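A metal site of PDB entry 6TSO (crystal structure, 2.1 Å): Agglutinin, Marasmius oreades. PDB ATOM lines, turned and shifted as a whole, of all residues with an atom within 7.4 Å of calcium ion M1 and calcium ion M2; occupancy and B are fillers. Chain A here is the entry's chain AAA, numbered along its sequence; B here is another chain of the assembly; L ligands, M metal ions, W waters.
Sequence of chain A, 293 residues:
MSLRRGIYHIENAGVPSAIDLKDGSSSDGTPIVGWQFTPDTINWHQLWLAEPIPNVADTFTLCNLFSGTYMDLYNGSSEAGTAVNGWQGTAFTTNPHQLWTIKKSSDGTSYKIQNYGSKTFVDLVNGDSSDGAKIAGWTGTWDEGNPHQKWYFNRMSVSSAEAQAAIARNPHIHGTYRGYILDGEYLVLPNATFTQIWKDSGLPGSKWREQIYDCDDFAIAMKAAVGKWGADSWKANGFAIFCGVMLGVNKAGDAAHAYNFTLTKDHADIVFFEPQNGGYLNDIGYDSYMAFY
N of Asp 214 lies within hydrogen-bond range of O of Arg 209, at 3.4 Å. N of Gly 184 of chain B is in hydrogen-bond range of OE1 of Gln 211, at 3.1 Å. The backbone NH of Asp 183 of chain B lies within hydrogen-bond range of the side-chain hydroxyl of Tyr 186 of chain B. N of Leu 182 of chain B lies within hydrogen-bond range of OXT of Tyr 293 of chain B (2.7 Å).
Within 4 Å of calcium ion M1: Asp 214, Asp 216, Leu 182 of chain B and Asp 183 of chain B.
Of the 24 residues printed, 5 come within 4 Å of calcium ion M2.
Calcium ion M1 is bound by the side-chain carboxylate (OD2) of Asp 214 (2.3 Å). The backbone carbonyl oxygen (O) of Leu 182 of chain B binds calcium ion M1, at 2.3 Å. Calcium ion M1 is bound by the side-chain carboxylate (OD1) of Asp 216, 2.4 Å away. Calcium ion M1 is bound by O1 of the ligand, 2.4 Å away. OD1 of Asp 183 of chain B is bound to calcium ion M1 (2.4 Å). Water W1 binds calcium ion M1 (2.5 Å).
OD1 of Asp 214 binds calcium ion M2 (2.3 Å). Calcium ion M2 is bound by OD2 of Asp 216 (2.3 Å). OD2 of Asp 217 binds calcium ion M2. Calcium ion M2 is bound by water W2, at 2.4 Å. Calcium ion M2 is bound by the backbone carbonyl oxygen (O) of Gln 211 (2.5 Å). Calcium ion M2 is bound by OD2 of Asp 183 of chain B, at 2.5 Å. OD1 of Asp 183 of chain B binds calcium ion M2, at 2.6 Å. Calcium ion M2 has seven donor atoms within binding distance.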
ATOM      1  N   TRP A 208      -6.364 -27.853  26.367  1.00  0.00           N
ATOM      2  CA  TRP A 208      -6.606 -26.438  26.007  1.00  0.00           C
ATOM      3  C   TRP A 208      -5.257 -25.803  25.679  1.00  0.00           C
ATOM      4  O   TRP A 208      -4.335 -25.810  26.534  1.00  0.00           O
ATOM      5  CB  TRP A 208      -7.303 -25.685  27.124  1.00  0.00           C
ATOM      6  CG  TRP A 208      -7.656 -24.280  26.727  1.00  0.00           C
ATOM      7  CD1 TRP A 208      -8.859 -23.836  26.272  1.00  0.00           C
ATOM      8  CD2 TRP A 208      -6.802 -23.129  26.796  1.00  0.00           C
ATOM      9  NE1 TRP A 208      -8.814 -22.487  26.039  1.00  0.00           N
ATOM     10  CE2 TRP A 208      -7.559 -22.033  26.340  1.00  0.00           C
ATOM     11  CE3 TRP A 208      -5.469 -22.918  27.191  1.00  0.00           C
ATOM     12  CZ2 TRP A 208      -7.036 -20.737  26.288  1.00  0.00           C
ATOM     13  CZ3 TRP A 208      -4.950 -21.648  27.125  1.00  0.00           C
ATOM     14  CH2 TRP A 208      -5.727 -20.565  26.689  1.00  0.00           C
ATOM     15  N   ARG A 209      -5.167 -25.263  24.476  1.00  0.00           N
ATOM     16  CA  ARG A 209      -4.009 -24.492  23.995  1.00  0.00           C
ATOM     17  C   ARG A 209      -4.570 -23.222  23.373  1.00  0.00           C
ATOM     18  O   ARG A 209      -5.480 -23.337  22.520  1.00  0.00           O
ATOM     19  CB  ARG A 209      -3.210 -25.355  23.010  1.00  0.00           C
ATOM     20  CG  ARG A 209      -2.644 -26.634  23.600  1.00  0.00           C
ATOM     21  CD  ARG A 209      -2.032 -27.579  22.564  1.00  0.00           C
ATOM     22  NE  ARG A 209      -1.041 -26.847  21.802  1.00  0.00           N
ATOM     23  CZ  ARG A 209      -0.506 -27.219  20.641  1.00  0.00           C
ATOM     24  NH1 ARG A 209      -0.824 -28.360  20.055  1.00  0.00           N
ATOM     25  NH2 ARG A 209       0.405 -26.414  20.103  1.00  0.00           N
ATOM     26  N   GLU A 210      -4.025 -22.075  23.778  1.00  0.00           N
ATOM     27  CA  GLU A 210      -4.397 -20.732  23.283  1.00  0.00           C
ATOM     28  C   GLU A 210      -4.503 -20.722  21.746  1.00  0.00           C
ATOM     29  O   GLU A 210      -3.473 -20.964  21.073  1.00  0.00           O
ATOM     30  CB  GLU A 210      -3.360 -19.715  23.741  1.00  0.00           C
ATOM     31  CG  GLU A 210      -3.898 -18.295  23.755  1.00  0.00           C
ATOM     32  CD  GLU A 210      -2.856 -17.288  24.182  1.00  0.00           C
ATOM     33  OE1 GLU A 210      -1.924 -17.681  24.906  1.00  0.00           O
ATOM     34  OE2 GLU A 210      -2.974 -16.115  23.773  1.00  0.00           O
ATOM     35  N   GLN A 211      -5.705 -20.443  21.242  1.00  0.00           N
ATOM     36  CA  GLN A 211      -6.097 -20.302  19.800  1.00  0.00           C
ATOM     37  C   GLN A 211      -5.918 -21.646  19.046  1.00  0.00           C
ATOM     38  O   GLN A 211      -6.829 -21.994  18.268  1.00  0.00           O
ATOM     39  CB  GLN A 211      -5.295 -19.167  19.158  1.00  0.00           C
ATOM     40  CG  GLN A 211      -5.648 -17.783  19.722  1.00  0.00           C
ATOM     41  CD  GLN A 211      -5.299 -16.641  18.783  1.00  0.00           C
ATOM     42  OE1 GLN A 211      -5.471 -16.734  17.570  1.00  0.00           O
ATOM     43  NE2 GLN A 211      -4.819 -15.542  19.337  1.00  0.00           N
ATOM     44  N   ILE A 212      -4.851 -22.427  19.278  1.00  0.00           N
ATOM     45  CA  ILE A 212      -4.534 -23.596  18.398  1.00  0.00           C
ATOM     46  C   ILE A 212      -5.478 -24.769  18.707  1.00  0.00           C
ATOM     47  O   ILE A 212      -5.797 -25.544  17.781  1.00  0.00           O
ATOM     48  CB  ILE A 212      -3.048 -23.991  18.548  1.00  0.00           C
ATOM     49  CG1 ILE A 212      -2.661 -24.959  17.428  1.00  0.00           C
ATOM     50  CG2 ILE A 212      -2.730 -24.556  19.926  1.00  0.00           C
ATOM     51  CD1 ILE A 212      -2.818 -24.377  16.069  1.00  0.00           C
ATOM     52  N   TYR A 213      -5.920 -24.878  19.958  1.00  0.00           N
ATOM     53  CA  TYR A 213      -6.936 -25.880  20.391  1.00  0.00           C
ATOM     54  C   TYR A 213      -7.607 -25.366  21.661  1.00  0.00           C
ATOM     55  O   TYR A 213      -7.315 -25.800  22.826  1.00  0.00           O
ATOM     56  CB  TYR A 213      -6.310 -27.251  20.607  1.00  0.00           C
ATOM     57  CG  TYR A 213      -7.216 -28.329  20.109  1.00  0.00           C
ATOM     58  CD1 TYR A 213      -7.406 -28.495  18.758  1.00  0.00           C
ATOM     59  CD2 TYR A 213      -7.964 -29.119  20.968  1.00  0.00           C
ATOM     60  CE1 TYR A 213      -8.284 -29.438  18.253  1.00  0.00           C
ATOM     61  CE2 TYR A 213      -8.842 -30.074  20.476  1.00  0.00           C
ATOM     62  CZ  TYR A 213      -8.998 -30.243  19.114  1.00  0.00           C
ATOM     63  OH  TYR A 213      -9.834 -31.185  18.564  1.00  0.00           O
ATOM     64  N   ASP A 214      -8.492 -24.413  21.451  1.00  0.00           N
ATOM     65  CA  ASP A 214      -9.195 -23.746  22.579  1.00  0.00           C
ATOM     66  C   ASP A 214     -10.670 -24.108  22.413  1.00  0.00           C
ATOM     67  O   ASP A 214     -10.958 -25.081  21.705  1.00  0.00           O
ATOM     68  CB  ASP A 214      -8.811 -22.275  22.564  1.00  0.00           C
ATOM     69  CG  ASP A 214      -9.368 -21.440  21.405  1.00  0.00           C
ATOM     70  OD1 ASP A 214      -9.364 -21.917  20.234  1.00  0.00           O
ATOM     71  OD2 ASP A 214      -9.711 -20.293  21.676  1.00  0.00           O
ATOM     72  N   CYS A 215     -11.574 -23.389  23.089  1.00  0.00           N
ATOM     73  CA  CYS A 215     -12.991 -23.811  23.273  1.00  0.00           C
ATOM     74  C   CYS A 215     -13.669 -23.997  21.900  1.00  0.00           C
ATOM     75  O   CYS A 215     -14.430 -25.011  21.749  1.00  0.00           O
ATOM     76  CB  CYS A 215     -13.757 -22.791  24.126  1.00  0.00           C
ATOM     77  SG  CYS A 215     -13.451 -21.063  23.703  1.00  0.00           S
ATOM     78  N   ASP A 216     -13.473 -23.104  20.927  1.00  0.00           N
ATOM     79  CA  ASP A 216     -14.094 -23.302  19.581  1.00  0.00           C
ATOM     80  C   ASP A 216     -13.638 -24.647  18.965  1.00  0.00           C
ATOM     81  O   ASP A 216     -14.454 -25.321  18.347  1.00  0.00           O
ATOM     82  CB  ASP A 216     -13.779 -22.182  18.594  1.00  0.00           C
ATOM     83  CG  ASP A 216     -12.337 -21.716  18.606  1.00  0.00           C
ATOM     84  OD1 ASP A 216     -11.956 -20.973  19.542  1.00  0.00           O
ATOM     85  OD2 ASP A 216     -11.597 -22.073  17.666  1.00  0.00           O
ATOM     86  N   ASP A 217     -12.358 -24.983  19.070  1.00  0.00           N
ATOM     87  CA  ASP A 217     -11.846 -26.269  18.519  1.00  0.00           C
ATOM     88  C   ASP A 217     -12.537 -27.451  19.233  1.00  0.00           C
ATOM     89  O   ASP A 217     -12.974 -28.387  18.521  1.00  0.00           O
ATOM     90  CB  ASP A 217     -10.324 -26.326  18.646  1.00  0.00           C
ATOM     91  CG  ASP A 217      -9.642 -25.222  17.835  1.00  0.00           C
ATOM     92  OD1 ASP A 217      -9.612 -25.356  16.599  1.00  0.00           O
ATOM     93  OD2 ASP A 217      -9.189 -24.233  18.433  1.00  0.00           O
ATOM     94  N   PHE A 218     -12.707 -27.414  20.557  1.00  0.00           N
ATOM     95  CA  PHE A 218     -13.354 -28.533  21.285  1.00  0.00           C
ATOM     96  C   PHE A 218     -14.832 -28.657  20.853  1.00  0.00           C
ATOM     97  O   PHE A 218     -15.296 -29.807  20.649  1.00  0.00           O
ATOM     98  CB  PHE A 218     -13.263 -28.388  22.802  1.00  0.00           C
ATOM     99  CG  PHE A 218     -11.940 -28.717  23.451  1.00  0.00           C
ATOM    100  CD1 PHE A 218     -10.891 -27.800  23.445  1.00  0.00           C
ATOM    101  CD2 PHE A 218     -11.775 -29.876  24.175  1.00  0.00           C
ATOM    102  CE1 PHE A 218      -9.703 -28.060  24.111  1.00  0.00           C
ATOM    103  CE2 PHE A 218     -10.572 -30.163  24.810  1.00  0.00           C
ATOM    104  CZ  PHE A 218      -9.542 -29.246  24.789  1.00  0.00           C
ATOM    105  N   ALA A 256     -15.888 -14.409  25.852  1.00  0.00           N
ATOM    106  CA  ALA A 256     -16.651 -15.327  24.972  1.00  0.00           C
ATOM    107  C   ALA A 256     -16.144 -16.760  25.175  1.00  0.00           C
ATOM    108  O   ALA A 256     -14.956 -16.971  25.465  1.00  0.00           O
ATOM    109  CB  ALA A 256     -16.547 -14.880  23.538  1.00  0.00           C
ATOM    110  N   ALA A 258     -17.081 -21.044  23.746  1.00  0.00           N
ATOM    111  CA  ALA A 258     -17.728 -21.998  22.825  1.00  0.00           C
ATOM    112  C   ALA A 258     -17.984 -23.310  23.579  1.00  0.00           C
ATOM    113  O   ALA A 258     -17.122 -23.754  24.412  1.00  0.00           O
ATOM    114  CB  ALA A 258     -16.873 -22.209  21.589  1.00  0.00           C
ATOM    115  N   ILE B 181     -16.296 -14.930  14.436  1.00  0.00           N
ATOM    116  CA  ILE B 181     -14.810 -14.952  14.502  1.00  0.00           C
ATOM    117  C   ILE B 181     -14.461 -15.832  15.695  1.00  0.00           C
ATOM    118  O   ILE B 181     -15.019 -15.594  16.765  1.00  0.00           O
ATOM    119  CB  ILE B 181     -14.208 -13.542  14.636  1.00  0.00           C
ATOM    120  CG1 ILE B 181     -14.273 -12.761  13.331  1.00  0.00           C
ATOM    121  CG2 ILE B 181     -12.785 -13.614  15.184  1.00  0.00           C
ATOM    122  CD1 ILE B 181     -15.647 -12.267  12.952  1.00  0.00           C
ATOM    123  N   LEU B 182     -13.578 -16.819  15.527  1.00  0.00           N
ATOM    124  CA  LEU B 182     -13.315 -17.791  16.628  1.00  0.00           C
ATOM    125  C   LEU B 182     -11.969 -17.483  17.266  1.00  0.00           C
ATOM    126  O   LEU B 182     -11.852 -17.707  18.460  1.00  0.00           O
ATOM    127  CB  LEU B 182     -13.335 -19.218  16.043  1.00  0.00           C
ATOM    128  CG  LEU B 182     -14.683 -19.596  15.422  1.00  0.00           C
ATOM    129  CD1 LEU B 182     -14.651 -21.014  14.851  1.00  0.00           C
ATOM    130  CD2 LEU B 182     -15.797 -19.456  16.435  1.00  0.00           C
ATOM    131  N   ASP B 183     -11.020 -16.954  16.499  1.00  0.00           N
ATOM    132  CA  ASP B 183      -9.601 -16.749  16.911  1.00  0.00           C
ATOM    133  C   ASP B 183      -9.111 -15.368  16.432  1.00  0.00           C
ATOM    134  O   ASP B 183      -9.895 -14.623  15.784  1.00  0.00           O
ATOM    135  CB  ASP B 183      -8.754 -17.910  16.407  1.00  0.00           C
ATOM    136  CG  ASP B 183      -9.141 -19.260  16.986  1.00  0.00           C
ATOM    137  OD1 ASP B 183      -9.162 -19.368  18.252  1.00  0.00           O
ATOM    138  OD2 ASP B 183      -9.490 -20.179  16.187  1.00  0.00           O
ATOM    139  N   GLY B 184      -7.867 -15.026  16.751  1.00  0.00           N
ATOM    140  CA  GLY B 184      -7.250 -13.713  16.461  1.00  0.00           C
ATOM    141  C   GLY B 184      -6.209 -13.725  15.346  1.00  0.00           C
ATOM    142  O   GLY B 184      -6.074 -12.696  14.695  1.00  0.00           O
ATOM    143  N   TYR B 186      -4.213 -16.363  12.272  1.00  0.00           N
ATOM    144  CA  TYR B 186      -4.489 -17.556  11.437  1.00  0.00           C
ATOM    145  C   TYR B 186      -3.351 -17.833  10.458  1.00  0.00           C
ATOM    146  O   TYR B 186      -3.096 -16.982   9.615  1.00  0.00           O
ATOM    147  CB  TYR B 186      -5.772 -17.370  10.657  1.00  0.00           C
ATOM    148  CG  TYR B 186      -7.020 -17.177  11.476  1.00  0.00           C
ATOM    149  CD1 TYR B 186      -7.762 -18.269  11.895  1.00  0.00           C
ATOM    150  CD2 TYR B 186      -7.475 -15.908  11.829  1.00  0.00           C
ATOM    151  CE1 TYR B 186      -8.919 -18.116  12.640  1.00  0.00           C
ATOM    152  CE2 TYR B 186      -8.624 -15.737  12.589  1.00  0.00           C
ATOM    153  CZ  TYR B 186      -9.362 -16.852  12.958  1.00  0.00           C
ATOM    154  OH  TYR B 186     -10.498 -16.722  13.691  1.00  0.00           O
ATOM    155  N   LYS B 223     -13.533 -28.371   8.611  1.00  0.00           N
ATOM    156  CA  LYS B 223     -13.014 -27.435   9.641  1.00  0.00           C
ATOM    157  C   LYS B 223     -12.409 -28.192  10.842  1.00  0.00           C
ATOM    158  O   LYS B 223     -11.384 -27.722  11.374  1.00  0.00           O
ATOM    159  CB  LYS B 223     -14.106 -26.530  10.205  1.00  0.00           C
ATOM    160  CG  LYS B 223     -13.544 -25.556  11.213  1.00  0.00           C
ATOM    161  CD  LYS B 223     -14.340 -24.281  11.320  1.00  0.00           C
ATOM    162  CE  LYS B 223     -13.762 -23.367  12.368  1.00  0.00           C
ATOM    163  NZ  LYS B 223     -12.344 -23.053  12.069  1.00  0.00           N
ATOM    164  N   GLY B 227      -8.459 -27.996  12.281  1.00  0.00           N
ATOM    165  CA  GLY B 227      -8.195 -27.723  13.714  1.00  0.00           C
ATOM    166  C   GLY B 227      -7.366 -28.852  14.336  1.00  0.00           C
ATOM    167  O   GLY B 227      -6.395 -28.574  15.047  1.00  0.00           O
ATOM    168  N   PHE B 239      -2.021 -19.022  18.086  1.00  0.00           N
ATOM    169  CA  PHE B 239      -2.481 -18.839  16.689  1.00  0.00           C
ATOM    170  C   PHE B 239      -3.425 -19.982  16.379  1.00  0.00           C
ATOM    171  O   PHE B 239      -3.364 -21.031  17.047  1.00  0.00           O
ATOM    172  CB  PHE B 239      -1.318 -18.820  15.689  1.00  0.00           C
ATOM    173  CG  PHE B 239      -0.595 -20.140  15.583  1.00  0.00           C
ATOM    174  CD1 PHE B 239       0.230 -20.566  16.607  1.00  0.00           C
ATOM    175  CD2 PHE B 239      -0.743 -20.944  14.469  1.00  0.00           C
ATOM    176  CE1 PHE B 239       0.892 -21.782  16.529  1.00  0.00           C
ATOM    177  CE2 PHE B 239      -0.106 -22.174  14.402  1.00  0.00           C
ATOM    178  CZ  PHE B 239       0.698 -22.601  15.433  1.00  0.00           C
ATOM    179  N   ALA B 240      -4.190 -19.815  15.309  1.00  0.00           N
ATOM    180  CA  ALA B 240      -5.071 -20.855  14.752  1.00  0.00           C
ATOM    181  C   ALA B 240      -4.702 -21.103  13.282  1.00  0.00           C
ATOM    182  O   ALA B 240      -3.858 -20.386  12.753  1.00  0.00           O
ATOM    183  CB  ALA B 240      -6.489 -20.433  14.896  1.00  0.00           C
ATOM    184  N   ILE B 241      -5.306 -22.127  12.665  1.00  0.00           N
ATOM    185  CA  ILE B 241      -5.161 -22.442  11.218  1.00  0.00           C
ATOM    186  C   ILE B 241      -6.401 -21.922  10.510  1.00  0.00           C
ATOM    187  O   ILE B 241      -7.504 -22.227  10.932  1.00  0.00           O
ATOM    188  CB  ILE B 241      -4.997 -23.946  10.989  1.00  0.00           C
ATOM    189  CG1 ILE B 241      -3.952 -24.544  11.938  1.00  0.00           C
ATOM    190  CG2 ILE B 241      -4.676 -24.211   9.528  1.00  0.00           C
ATOM    191  CD1 ILE B 241      -2.595 -23.860  11.939  1.00  0.00           C
ATOM    192  N   TYR B 293     -15.060 -19.014  11.299  1.00  0.00           N
ATOM    193  CA  TYR B 293     -13.604 -19.111  11.036  1.00  0.00           C
ATOM    194  C   TYR B 293     -12.868 -18.668  12.301  1.00  0.00           C
ATOM    195  O   TYR B 293     -11.819 -19.223  12.627  1.00  0.00           O
ATOM    196  CB  TYR B 293     -13.219 -18.260   9.819  1.00  0.00           C
ATOM    197  CG  TYR B 293     -13.601 -16.803   9.838  1.00  0.00           C
ATOM    198  CD1 TYR B 293     -14.802 -16.372   9.289  1.00  0.00           C
ATOM    199  CD2 TYR B 293     -12.750 -15.842  10.337  1.00  0.00           C
ATOM    200  CE1 TYR B 293     -15.149 -15.035   9.281  1.00  0.00           C
ATOM    201  CE2 TYR B 293     -13.073 -14.501  10.332  1.00  0.00           C
ATOM    202  CZ  TYR B 293     -14.272 -14.092   9.786  1.00  0.00           C
ATOM    203  OH  TYR B 293     -14.595 -12.765   9.762  1.00  0.00           O
ATOM    204  OXT TYR B 293     -13.340 -17.776  13.024  1.00  0.00           O
HETATM  205  C1  LIG L   1     -13.772 -17.905  21.795  1.00  0.00           C
HETATM  206  O1  LIG L   1     -12.475 -18.425  21.668  1.00  0.00           O
HETATM  207  C2  LIG L   1     -14.603 -18.192  20.612  1.00  0.00           C
HETATM  208  O2  LIG L   1     -15.971 -18.193  20.911  1.00  0.00           O
HETATM  209 CA    CA M   1     -10.766 -19.002  20.058  1.00  0.00          CA
HETATM  210 CA    CA M   2      -9.292 -21.936  17.949  1.00  0.00          CA
HETATM  211 CD    CD M   3     -13.136 -20.460  26.152  1.00  0.00          CD
HETATM  212  O   HOH W   1      -9.332 -17.020  20.656  1.00  0.00           O
HETATM  213  O   HOH W   2      -9.029 -23.148  15.850  1.00  0.00           O
